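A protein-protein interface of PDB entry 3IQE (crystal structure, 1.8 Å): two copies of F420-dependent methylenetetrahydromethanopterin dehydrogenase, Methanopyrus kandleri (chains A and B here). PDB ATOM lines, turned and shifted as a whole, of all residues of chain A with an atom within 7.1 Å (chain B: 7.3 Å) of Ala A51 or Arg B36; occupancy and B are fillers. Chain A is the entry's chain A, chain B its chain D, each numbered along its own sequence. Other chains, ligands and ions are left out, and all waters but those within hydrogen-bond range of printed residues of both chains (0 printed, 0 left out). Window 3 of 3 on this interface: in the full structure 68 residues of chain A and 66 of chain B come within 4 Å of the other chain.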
ATOM      1  N   CYS A  11      14.899  -0.721 -13.806  1.00  0.00           N
ATOM      2  CA  CYS A  11      15.335  -1.113 -12.459  1.00  0.00           C
ATOM      3  C   CYS A  11      14.196  -0.897 -11.501  1.00  0.00           C
ATOM      4  O   CYS A  11      13.721   0.225 -11.338  1.00  0.00           O
ATOM      5  CB  CYS A  11      16.532  -0.294 -12.007  1.00  0.00           C
ATOM      6  SG  CYS A  11      17.969  -0.577 -13.020  1.00  0.00           S
ATOM      7  N   VAL A  38      17.679  -3.298 -21.190  1.00  0.00           N
ATOM      8  CA  VAL A  38      18.518  -3.966 -20.203  1.00  0.00           C
ATOM      9  C   VAL A  38      18.050  -3.579 -18.810  1.00  0.00           C
ATOM     10  O   VAL A  38      17.360  -2.584 -18.619  1.00  0.00           O
ATOM     11  CB  VAL A  38      20.048  -3.691 -20.374  1.00  0.00           C
ATOM     12  CG1 VAL A  38      20.488  -3.902 -21.839  1.00  0.00           C
ATOM     13  CG2 VAL A  38      20.445  -2.299 -19.897  1.00  0.00           C
ATOM     14  N   GLY A  39      18.412  -4.386 -17.835  1.00  0.00           N
ATOM     15  CA  GLY A  39      18.010  -4.093 -16.490  1.00  0.00           C
ATOM     16  C   GLY A  39      18.457  -5.114 -15.475  1.00  0.00           C
ATOM     17  O   GLY A  39      19.113  -6.092 -15.804  1.00  0.00           O
ATOM     18  N   THR A  40      18.031  -4.887 -14.242  1.00  0.00           N
ATOM     19  CA  THR A  40      18.342  -5.757 -13.120  1.00  0.00           C
ATOM     20  C   THR A  40      17.066  -6.223 -12.446  1.00  0.00           C
ATOM     21  O   THR A  40      17.043  -6.469 -11.238  1.00  0.00           O
ATOM     22  CB  THR A  40      19.182  -5.026 -12.027  1.00  0.00           C
ATOM     23  OG1 THR A  40      18.542  -3.808 -11.645  1.00  0.00           O
ATOM     24  CG2 THR A  40      20.579  -4.708 -12.517  1.00  0.00           C
ATOM     25  N   SER A  41      15.986  -6.321 -13.214  1.00  0.00           N
ATOM     26  CA  SER A  41      14.727  -6.780 -12.654  1.00  0.00           C
ATOM     27  C   SER A  41      14.250  -5.832 -11.534  1.00  0.00           C
ATOM     28  O   SER A  41      14.451  -4.623 -11.613  1.00  0.00           O
ATOM     29  CB  SER A  41      14.913  -8.193 -12.119  1.00  0.00           C
ATOM     30  OG  SER A  41      13.677  -8.817 -11.873  1.00  0.00           O
ATOM     31  N   ASP A  45      18.598  -0.981  -5.730  1.00  0.00           N
ATOM     32  CA  ASP A  45      19.598  -0.468  -4.799  1.00  0.00           C
ATOM     33  C   ASP A  45      20.748   0.159  -5.602  1.00  0.00           C
ATOM     34  O   ASP A  45      20.883  -0.102  -6.782  1.00  0.00           O
ATOM     35  CB  ASP A  45      20.135  -1.637  -3.976  1.00  0.00           C
ATOM     36  CG  ASP A  45      20.726  -2.739  -4.856  1.00  0.00           C
ATOM     37  OD1 ASP A  45      19.963  -3.564  -5.430  1.00  0.00           O
ATOM     38  OD2 ASP A  45      21.973  -2.774  -4.981  1.00  0.00           O
ATOM     39  N   PRO A  46      21.585   0.999  -4.968  1.00  0.00           N
ATOM     40  CA  PRO A  46      22.668   1.634  -5.733  1.00  0.00           C
ATOM     41  C   PRO A  46      23.628   0.673  -6.458  1.00  0.00           C
ATOM     42  O   PRO A  46      24.084   0.991  -7.545  1.00  0.00           O
ATOM     43  CB  PRO A  46      23.411   2.450  -4.673  1.00  0.00           C
ATOM     44  CG  PRO A  46      22.359   2.812  -3.693  1.00  0.00           C
ATOM     45  CD  PRO A  46      21.363   1.665  -3.674  1.00  0.00           C
ATOM     46  N   GLU A  47      23.924  -0.485  -5.875  1.00  0.00           N
ATOM     47  CA  GLU A  47      24.835  -1.439  -6.509  1.00  0.00           C
ATOM     48  C   GLU A  47      24.285  -1.923  -7.844  1.00  0.00           C
ATOM     49  O   GLU A  47      24.995  -1.983  -8.846  1.00  0.00           O
ATOM     50  CB  GLU A  47      25.043  -2.671  -5.627  1.00  0.00           C
ATOM     51  CG  GLU A  47      25.767  -2.402  -4.320  1.00  0.00           C
ATOM     52  CD  GLU A  47      24.846  -1.826  -3.255  1.00  0.00           C
ATOM     53  OE1 GLU A  47      23.623  -1.668  -3.519  1.00  0.00           O
ATOM     54  OE2 GLU A  47      25.354  -1.529  -2.151  1.00  0.00           O
ATOM     55  N   CYS A  48      23.015  -2.297  -7.808  1.00  0.00           N
ATOM     56  CA  CYS A  48      22.337  -2.913  -8.942  1.00  0.00           C
ATOM     57  C   CYS A  48      22.042  -1.897 -10.007  1.00  0.00           C
ATOM     58  O   CYS A  48      22.103  -2.200 -11.203  1.00  0.00           O
ATOM     59  CB  CYS A  48      21.031  -3.558  -8.497  1.00  0.00           C
ATOM     60  SG  CYS A  48      21.255  -4.861  -7.285  1.00  0.00           S
ATOM     61  N   VAL A  49      21.717  -0.689  -9.582  1.00  0.00           N
ATOM     62  CA  VAL A  49      21.400   0.352 -10.549  1.00  0.00           C
ATOM     63  C   VAL A  49      22.700   0.769 -11.266  1.00  0.00           C
ATOM     64  O   VAL A  49      22.724   0.888 -12.488  1.00  0.00           O
ATOM     65  CB  VAL A  49      20.656   1.556  -9.902  1.00  0.00           C
ATOM     66  CG1 VAL A  49      20.590   2.687 -10.866  1.00  0.00           C
ATOM     67  CG2 VAL A  49      19.219   1.154  -9.447  1.00  0.00           C
ATOM     68  N   GLU A  50      23.810   0.950 -10.545  1.00  0.00           N
ATOM     69  CA  GLU A  50      25.052   1.205 -11.257  1.00  0.00           C
ATOM     70  C   GLU A  50      25.255   0.080 -12.280  1.00  0.00           C
ATOM     71  O   GLU A  50      25.436   0.336 -13.466  1.00  0.00           O
ATOM     72  CB  GLU A  50      26.267   1.321 -10.317  1.00  0.00           C
ATOM     73  CG  GLU A  50      27.623   1.499 -11.069  1.00  0.00           C
ATOM     74  CD  GLU A  50      28.764   1.951 -10.165  1.00  0.00           C
ATOM     75  OE1 GLU A  50      29.954   1.780 -10.539  1.00  0.00           O
ATOM     76  OE2 GLU A  50      28.475   2.488  -9.070  1.00  0.00           O
ATOM     77  N   ALA A  51      25.201  -1.168 -11.823  1.00  0.00           N
ATOM     78  CA  ALA A  51      25.456  -2.313 -12.692  1.00  0.00           C
ATOM     79  C   ALA A  51      24.623  -2.254 -13.962  1.00  0.00           C
ATOM     80  O   ALA A  51      25.075  -2.625 -15.035  1.00  0.00           O
ATOM     81  CB  ALA A  51      25.162  -3.593 -11.956  1.00  0.00           C
ATOM     82  N   ALA A  52      23.397  -1.776 -13.830  1.00  0.00           N
ATOM     83  CA  ALA A  52      22.477  -1.725 -14.954  1.00  0.00           C
ATOM     84  C   ALA A  52      22.788  -0.601 -15.926  1.00  0.00           C
ATOM     85  O   ALA A  52      22.663  -0.782 -17.144  1.00  0.00           O
ATOM     86  CB  ALA A  52      21.088  -1.567 -14.442  1.00  0.00           C
ATOM     87  N   VAL A  53      23.150   0.569 -15.402  1.00  0.00           N
ATOM     88  CA  VAL A  53      23.496   1.698 -16.266  1.00  0.00           C
ATOM     89  C   VAL A  53      24.837   1.431 -16.952  1.00  0.00           C
ATOM     90  O   VAL A  53      25.049   1.762 -18.125  1.00  0.00           O
ATOM     91  CB  VAL A  53      23.530   3.021 -15.492  1.00  0.00           C
ATOM     92  CG1 VAL A  53      24.039   4.137 -16.382  1.00  0.00           C
ATOM     93  CG2 VAL A  53      22.149   3.348 -14.960  1.00  0.00           C
ATOM     94  N   GLU A  54      25.739   0.782 -16.233  1.00  0.00           N
ATOM     95  CA  GLU A  54      27.018   0.410 -16.828  1.00  0.00           C
ATOM     96  C   GLU A  54      26.781  -0.490 -18.022  1.00  0.00           C
ATOM     97  O   GLU A  54      27.277  -0.233 -19.125  1.00  0.00           O
ATOM     98  CB  GLU A  54      27.881  -0.294 -15.793  1.00  0.00           C
ATOM     99  CG  GLU A  54      29.353  -0.060 -15.981  1.00  0.00           C
ATOM    100  CD  GLU A  54      30.067   0.143 -14.655  1.00  0.00           C
ATOM    101  OE1 GLU A  54      29.721   1.098 -13.927  1.00  0.00           O
ATOM    102  OE2 GLU A  54      30.974  -0.649 -14.339  1.00  0.00           O
ATOM    103  N   MET A  55      26.006  -1.549 -17.809  1.00  0.00           N
ATOM    104  CA  MET A  55      25.590  -2.403 -18.910  1.00  0.00           C
ATOM    105  C   MET A  55      25.113  -1.565 -20.089  1.00  0.00           C
ATOM    106  O   MET A  55      25.611  -1.713 -21.199  1.00  0.00           O
ATOM    107  CB  MET A  55      24.445  -3.312 -18.484  1.00  0.00           C
ATOM    108  CG  MET A  55      24.827  -4.662 -17.938  1.00  0.00           C
ATOM    109  SD  MET A  55      23.356  -5.727 -17.918  1.00  0.00           S
ATOM    110  CE  MET A  55      22.168  -4.693 -17.068  1.00  0.00           C
ATOM    111  N   ALA A  56      24.156  -0.678 -19.844  1.00  0.00           N
ATOM    112  CA  ALA A  56      23.564   0.129 -20.913  1.00  0.00           C
ATOM    113  C   ALA A  56      24.610   0.997 -21.614  1.00  0.00           C
ATOM    114  O   ALA A  56      24.608   1.151 -22.829  1.00  0.00           O
ATOM    115  CB  ALA A  56      22.465   0.999 -20.358  1.00  0.00           C
ATOM    116  N   LYS A  82      21.459   7.622  -8.340  1.00  0.00           N
ATOM    117  CA  LYS A  82      22.747   7.222  -8.911  1.00  0.00           C
ATOM    118  C   LYS A  82      22.652   7.197 -10.431  1.00  0.00           C
ATOM    119  O   LYS A  82      23.548   7.662 -11.115  1.00  0.00           O
ATOM    120  CB  LYS A  82      23.182   5.864  -8.356  1.00  0.00           C
ATOM    121  CG  LYS A  82      24.397   5.209  -9.052  1.00  0.00           C
ATOM    122  CD  LYS A  82      25.694   5.964  -8.831  1.00  0.00           C
ATOM    123  CE  LYS A  82      26.879   5.235  -9.485  1.00  0.00           C
ATOM    124  NZ  LYS A  82      28.163   5.972  -9.298  1.00  0.00           N
ATOM    125  N   MET A  86      24.778   9.339 -13.401  1.00  0.00           N
ATOM    126  CA  MET A  86      25.561   8.694 -14.454  1.00  0.00           C
ATOM    127  C   MET A  86      25.025   9.105 -15.811  1.00  0.00           C
ATOM    128  O   MET A  86      25.772   9.418 -16.708  1.00  0.00           O
ATOM    129  CB  MET A  86      25.557   7.169 -14.340  1.00  0.00           C
ATOM    130  CG  MET A  86      26.016   6.633 -13.013  1.00  0.00           C
ATOM    131  SD  MET A  86      25.748   4.855 -12.853  1.00  0.00           S
ATOM    132  CE  MET A  86      26.940   4.227 -14.036  1.00  0.00           C
ATOM    133  N   LYS B   5      22.384 -17.027  -9.601  1.00  0.00           N
ATOM    134  CA  LYS B   5      22.366 -15.939 -10.563  1.00  0.00           C
ATOM    135  C   LYS B   5      21.749 -16.408 -11.895  1.00  0.00           C
ATOM    136  O   LYS B   5      21.932 -17.561 -12.290  1.00  0.00           O
ATOM    137  CB  LYS B   5      23.785 -15.380 -10.740  1.00  0.00           C
ATOM    138  CG  LYS B   5      24.297 -14.607  -9.508  1.00  0.00           C
ATOM    139  CD  LYS B   5      25.741 -14.172  -9.636  1.00  0.00           C
ATOM    140  CE  LYS B   5      26.668 -15.183  -8.996  1.00  0.00           C
ATOM    141  NZ  LYS B   5      28.119 -14.949  -9.345  1.00  0.00           N
ATOM    142  N   ALA B   6      21.019 -15.522 -12.584  1.00  0.00           N
ATOM    143  CA  ALA B   6      20.341 -15.885 -13.830  1.00  0.00           C
ATOM    144  C   ALA B   6      20.203 -14.698 -14.784  1.00  0.00           C
ATOM    145  O   ALA B   6      20.105 -13.540 -14.357  1.00  0.00           O
ATOM    146  CB  ALA B   6      18.956 -16.468 -13.520  1.00  0.00           C
ATOM    147  N   ILE B   7      20.209 -14.981 -16.088  1.00  0.00           N
ATOM    148  CA  ILE B   7      20.006 -13.920 -17.062  1.00  0.00           C
ATOM    149  C   ILE B   7      18.762 -14.265 -17.816  1.00  0.00           C
ATOM    150  O   ILE B   7      18.589 -15.409 -18.241  1.00  0.00           O
ATOM    151  CB  ILE B   7      21.176 -13.785 -18.057  1.00  0.00           C
ATOM    152  CG1 ILE B   7      22.522 -13.537 -17.354  1.00  0.00           C
ATOM    153  CG2 ILE B   7      20.895 -12.672 -19.032  1.00  0.00           C
ATOM    154  CD1 ILE B   7      23.685 -13.417 -18.330  1.00  0.00           C
ATOM    155  N   PHE B   8      17.868 -13.293 -17.937  1.00  0.00           N
ATOM    156  CA  PHE B   8      16.648 -13.468 -18.700  1.00  0.00           C
ATOM    157  C   PHE B   8      16.810 -12.725 -20.004  1.00  0.00           C
ATOM    158  O   PHE B   8      17.298 -11.616 -20.008  1.00  0.00           O
ATOM    159  CB  PHE B   8      15.493 -12.879 -17.939  1.00  0.00           C
ATOM    160  CG  PHE B   8      15.155 -13.623 -16.667  1.00  0.00           C
ATOM    161  CD1 PHE B   8      15.849 -13.368 -15.482  1.00  0.00           C
ATOM    162  CD2 PHE B   8      14.152 -14.589 -16.661  1.00  0.00           C
ATOM    163  CE1 PHE B   8      15.521 -14.062 -14.304  1.00  0.00           C
ATOM    164  CE2 PHE B   8      13.809 -15.284 -15.491  1.00  0.00           C
ATOM    165  CZ  PHE B   8      14.509 -15.028 -14.316  1.00  0.00           C
ATOM    166  N   ILE B   9      16.388 -13.330 -21.105  1.00  0.00           N
ATOM    167  CA  ILE B   9      16.480 -12.695 -22.427  1.00  0.00           C
ATOM    168  C   ILE B   9      15.061 -12.568 -22.926  1.00  0.00           C
ATOM    169  O   ILE B   9      14.330 -13.545 -22.928  1.00  0.00           O
ATOM    170  CB  ILE B   9      17.222 -13.542 -23.462  1.00  0.00           C
ATOM    171  CG1 ILE B   9      18.656 -13.796 -23.025  1.00  0.00           C
ATOM    172  CG2 ILE B   9      17.212 -12.829 -24.798  1.00  0.00           C
ATOM    173  CD1 ILE B   9      19.206 -15.165 -23.414  1.00  0.00           C
ATOM    174  N   ASP B  21      10.642 -12.861 -14.388  1.00  0.00           N
ATOM    175  CA  ASP B  21      11.672 -12.560 -13.385  1.00  0.00           C
ATOM    176  C   ASP B  21      11.070 -11.969 -12.107  1.00  0.00           C
ATOM    177  O   ASP B  21      11.500 -12.266 -10.998  1.00  0.00           O
ATOM    178  CB  ASP B  21      12.759 -11.637 -13.954  1.00  0.00           C
ATOM    179  CG  ASP B  21      12.195 -10.355 -14.568  1.00  0.00           C
ATOM    180  OD1 ASP B  21      11.423 -10.456 -15.557  1.00  0.00           O
ATOM    181  OD2 ASP B  21      12.520  -9.255 -14.055  1.00  0.00           O
ATOM    182  N   GLU B  34      20.312 -13.075  -7.904  1.00  0.00           N
ATOM    183  CA  GLU B  34      20.626 -11.874  -8.640  1.00  0.00           C
ATOM    184  C   GLU B  34      20.359 -12.074 -10.129  1.00  0.00           C
ATOM    185  O   GLU B  34      20.780 -13.083 -10.713  1.00  0.00           O
ATOM    186  CB  GLU B  34      22.087 -11.529  -8.436  1.00  0.00           C
ATOM    187  CG  GLU B  34      22.345 -10.143  -7.889  1.00  0.00           C
ATOM    188  CD  GLU B  34      23.768  -9.673  -8.160  1.00  0.00           C
ATOM    189  OE1 GLU B  34      23.928  -8.815  -9.059  1.00  0.00           O
ATOM    190  OE2 GLU B  34      24.722 -10.153  -7.499  1.00  0.00           O
ATOM    191  N   PHE B  35      19.685 -11.099 -10.739  1.00  0.00           N
ATOM    192  CA  PHE B  35      19.226 -11.229 -12.112  1.00  0.00           C
ATOM    193  C   PHE B  35      19.765 -10.112 -12.989  1.00  0.00           C
ATOM    194  O   PHE B  35      19.967  -9.000 -12.527  1.00  0.00           O
ATOM    195  CB  PHE B  35      17.706 -11.199 -12.139  1.00  0.00           C
ATOM    196  CG  PHE B  35      17.076 -12.311 -11.345  1.00  0.00           C
ATOM    197  CD1 PHE B  35      15.979 -12.076 -10.540  1.00  0.00           C
ATOM    198  CD2 PHE B  35      17.608 -13.592 -11.395  1.00  0.00           C
ATOM    199  CE1 PHE B  35      15.410 -13.105  -9.804  1.00  0.00           C
ATOM    200  CE2 PHE B  35      17.055 -14.629 -10.656  1.00  0.00           C
ATOM    201  CZ  PHE B  35      15.953 -14.392  -9.868  1.00  0.00           C
ATOM    202  N   ARG B  36      20.003 -10.424 -14.256  1.00  0.00           N
ATOM    203  CA  ARG B  36      20.157  -9.427 -15.289  1.00  0.00           C
ATOM    204  C   ARG B  36      19.083  -9.754 -16.323  1.00  0.00           C
ATOM    205  O   ARG B  36      18.728 -10.911 -16.500  1.00  0.00           O
ATOM    206  CB  ARG B  36      21.548  -9.483 -15.912  1.00  0.00           C
ATOM    207  CG  ARG B  36      22.660  -9.168 -14.914  1.00  0.00           C
ATOM    208  CD  ARG B  36      22.685  -7.690 -14.564  1.00  0.00           C
ATOM    209  NE  ARG B  36      23.817  -7.399 -13.694  1.00  0.00           N
ATOM    210  CZ  ARG B  36      23.830  -7.643 -12.394  1.00  0.00           C
ATOM    211  NH1 ARG B  36      24.912  -7.365 -11.686  1.00  0.00           N
ATOM    212  NH2 ARG B  36      22.780  -8.173 -11.800  1.00  0.00           N
ATOM    213  N   VAL B  37      18.560  -8.724 -16.962  1.00  0.00           N
ATOM    214  CA  VAL B  37      17.557  -8.871 -17.989  1.00  0.00           C
ATOM    215  C   VAL B  37      18.069  -8.129 -19.206  1.00  0.00           C
ATOM    216  O   VAL B  37      18.525  -6.992 -19.085  1.00  0.00           O
ATOM    217  CB  VAL B  37      16.227  -8.238 -17.559  1.00  0.00           C
ATOM    218  CG1 VAL B  37      15.151  -8.408 -18.658  1.00  0.00           C
ATOM    219  CG2 VAL B  37      15.739  -8.843 -16.255  1.00  0.00           C
ATOM    220  N   VAL B  38      17.979  -8.752 -20.374  1.00  0.00           N
ATOM    221  CA  VAL B  38      18.359  -8.093 -21.605  1.00  0.00           C
ATOM    222  C   VAL B  38      17.376  -8.487 -22.699  1.00  0.00           C
ATOM    223  O   VAL B  38      16.891  -9.589 -22.686  1.00  0.00           O
ATOM    224  CB  VAL B  38      19.778  -8.486 -22.020  1.00  0.00           C
ATOM    225  CG1 VAL B  38      20.729  -8.020 -20.972  1.00  0.00           C
ATOM    226  CG2 VAL B  38      19.900  -9.997 -22.224  1.00  0.00           C
ATOM    227  N   ILE B  59      27.494 -10.558 -21.300  1.00  0.00           N
ATOM    228  CA  ILE B  59      27.322 -10.185 -19.909  1.00  0.00           C
ATOM    229  C   ILE B  59      27.636 -11.343 -18.974  1.00  0.00           C
ATOM    230  O   ILE B  59      28.094 -11.137 -17.842  1.00  0.00           O
ATOM    231  CB  ILE B  59      25.895  -9.705 -19.654  1.00  0.00           C
ATOM    232  CG1 ILE B  59      25.717  -8.316 -20.270  1.00  0.00           C
ATOM    233  CG2 ILE B  59      25.615  -9.691 -18.167  1.00  0.00           C
ATOM    234  CD1 ILE B  59      24.275  -7.970 -20.553  1.00  0.00           C
ATOM    235  N   PHE B  63      29.406 -12.102 -15.256  1.00  0.00           N
ATOM    236  CA  PHE B  63      28.325 -12.336 -14.291  1.00  0.00           C
ATOM    237  C   PHE B  63      28.262 -13.792 -13.787  1.00  0.00           C
ATOM    238  O   PHE B  63      27.901 -14.025 -12.629  1.00  0.00           O
ATOM    239  CB  PHE B  63      27.002 -11.924 -14.939  1.00  0.00           C
ATOM    240  CG  PHE B  63      25.818 -11.905 -14.000  1.00  0.00           C
ATOM    241  CD1 PHE B  63      25.807 -11.091 -12.878  1.00  0.00           C
ATOM    242  CD2 PHE B  63      24.698 -12.678 -14.262  1.00  0.00           C
ATOM    243  CE1 PHE B  63      24.713 -11.066 -12.020  1.00  0.00           C
ATOM    244  CE2 PHE B  63      23.588 -12.648 -13.395  1.00  0.00           C
ATOM    245  CZ  PHE B  63      23.605 -11.846 -12.286  1.00  0.00           C
ATOM    246  N   VAL B  69      17.516 -17.837 -19.141  1.00  0.00           N
ATOM    247  CA  VAL B  69      16.135 -18.058 -19.524  1.00  0.00           C
ATOM    248  C   VAL B  69      15.865 -17.216 -20.743  1.00  0.00           C
ATOM    249  O   VAL B  69      16.159 -16.035 -20.724  1.00  0.00           O
ATOM    250  CB  VAL B  69      15.155 -17.620 -18.424  1.00  0.00           C
ATOM    251  CG1 VAL B  69      13.685 -17.874 -18.883  1.00  0.00           C
ATOM    252  CG2 VAL B  69      15.426 -18.362 -17.168  1.00  0.00           C
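N of Gly A39 is in hydrogen-bond range of O of Val B37, at 2.9 Å. The side-chain carboxylate of Asp B21 sits at hydrogen-bond distance from the side-chain hydroxyl of Ser A41 (2.5 Å).
SG of Cys A11 is in hydrogen-bond range of OG1 of Thr A40 (3.6 Å). The backbone carbonyl oxygen (O) of Ala B6 sits at hydrogen-bond distance from the backbone NH (N) of Arg B36 (3.1 Å). The backbone carbonyl oxygen (O) of Arg B36 is in hydrogen-bond range of the backbone NH (N) of Phe B8, 2.9 Å away. The guanidinium group (NH2) of Arg B36 lies within salt-bridge range of the side-chain carboxylate (OE1) of Glu B34.
Val A38 touches Val B37 (CA to O, 3.2 Å). Arg B36 touches Gly A39 (CA to O, 3.5 Å). Phe B35 touches Thr A40 (O to CA, 3.7 Å). N of Ser A41 touches CG2 of Val B37, at 3.96 Å. NH1 of Arg B36 touches CB of Ala A51, at 3.8 Å. Met A55 touches Arg B36 (CE to CD, 3.9 Å). Met A55 touches Ile B59.
Ala A51 touches just one residue of chain B: Arg B36. Arg B36 touches just these residues of chain A: Gly A39 (3.5 Å), Ala A51 (3.8 Å) and Met A55 (3.9 Å). Of the printed residues of chain B, Met A55 touches Arg B36 and Ile B59. Of the printed residues of chain B, Val A38 touches Val B37 (3.2 Å). Of the printed residues of chain A, Val B37 touches Val A38, Gly A39 and Ser A41. Lys A82 touches none of the printed residues of chain B.
Hydrophobic or aromatic side chains of chain A within 4 Å of the printed part of chain B: Val A38, Ala A51 and Met A55. Hydrophobic or aromatic side chains of chain B within 4 Å of the printed part of chain A: Val B37 and Ile B59. Among the printed residues, no Asp or Glu carboxylate lies within 4 Å of a Lys or Arg side-chain nitrogen of the other chain.
Position printed for both chains: 38. Of the 9 pairs that touch across the chains among the printed residues, none has its exchanged pair printed and touching as well.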
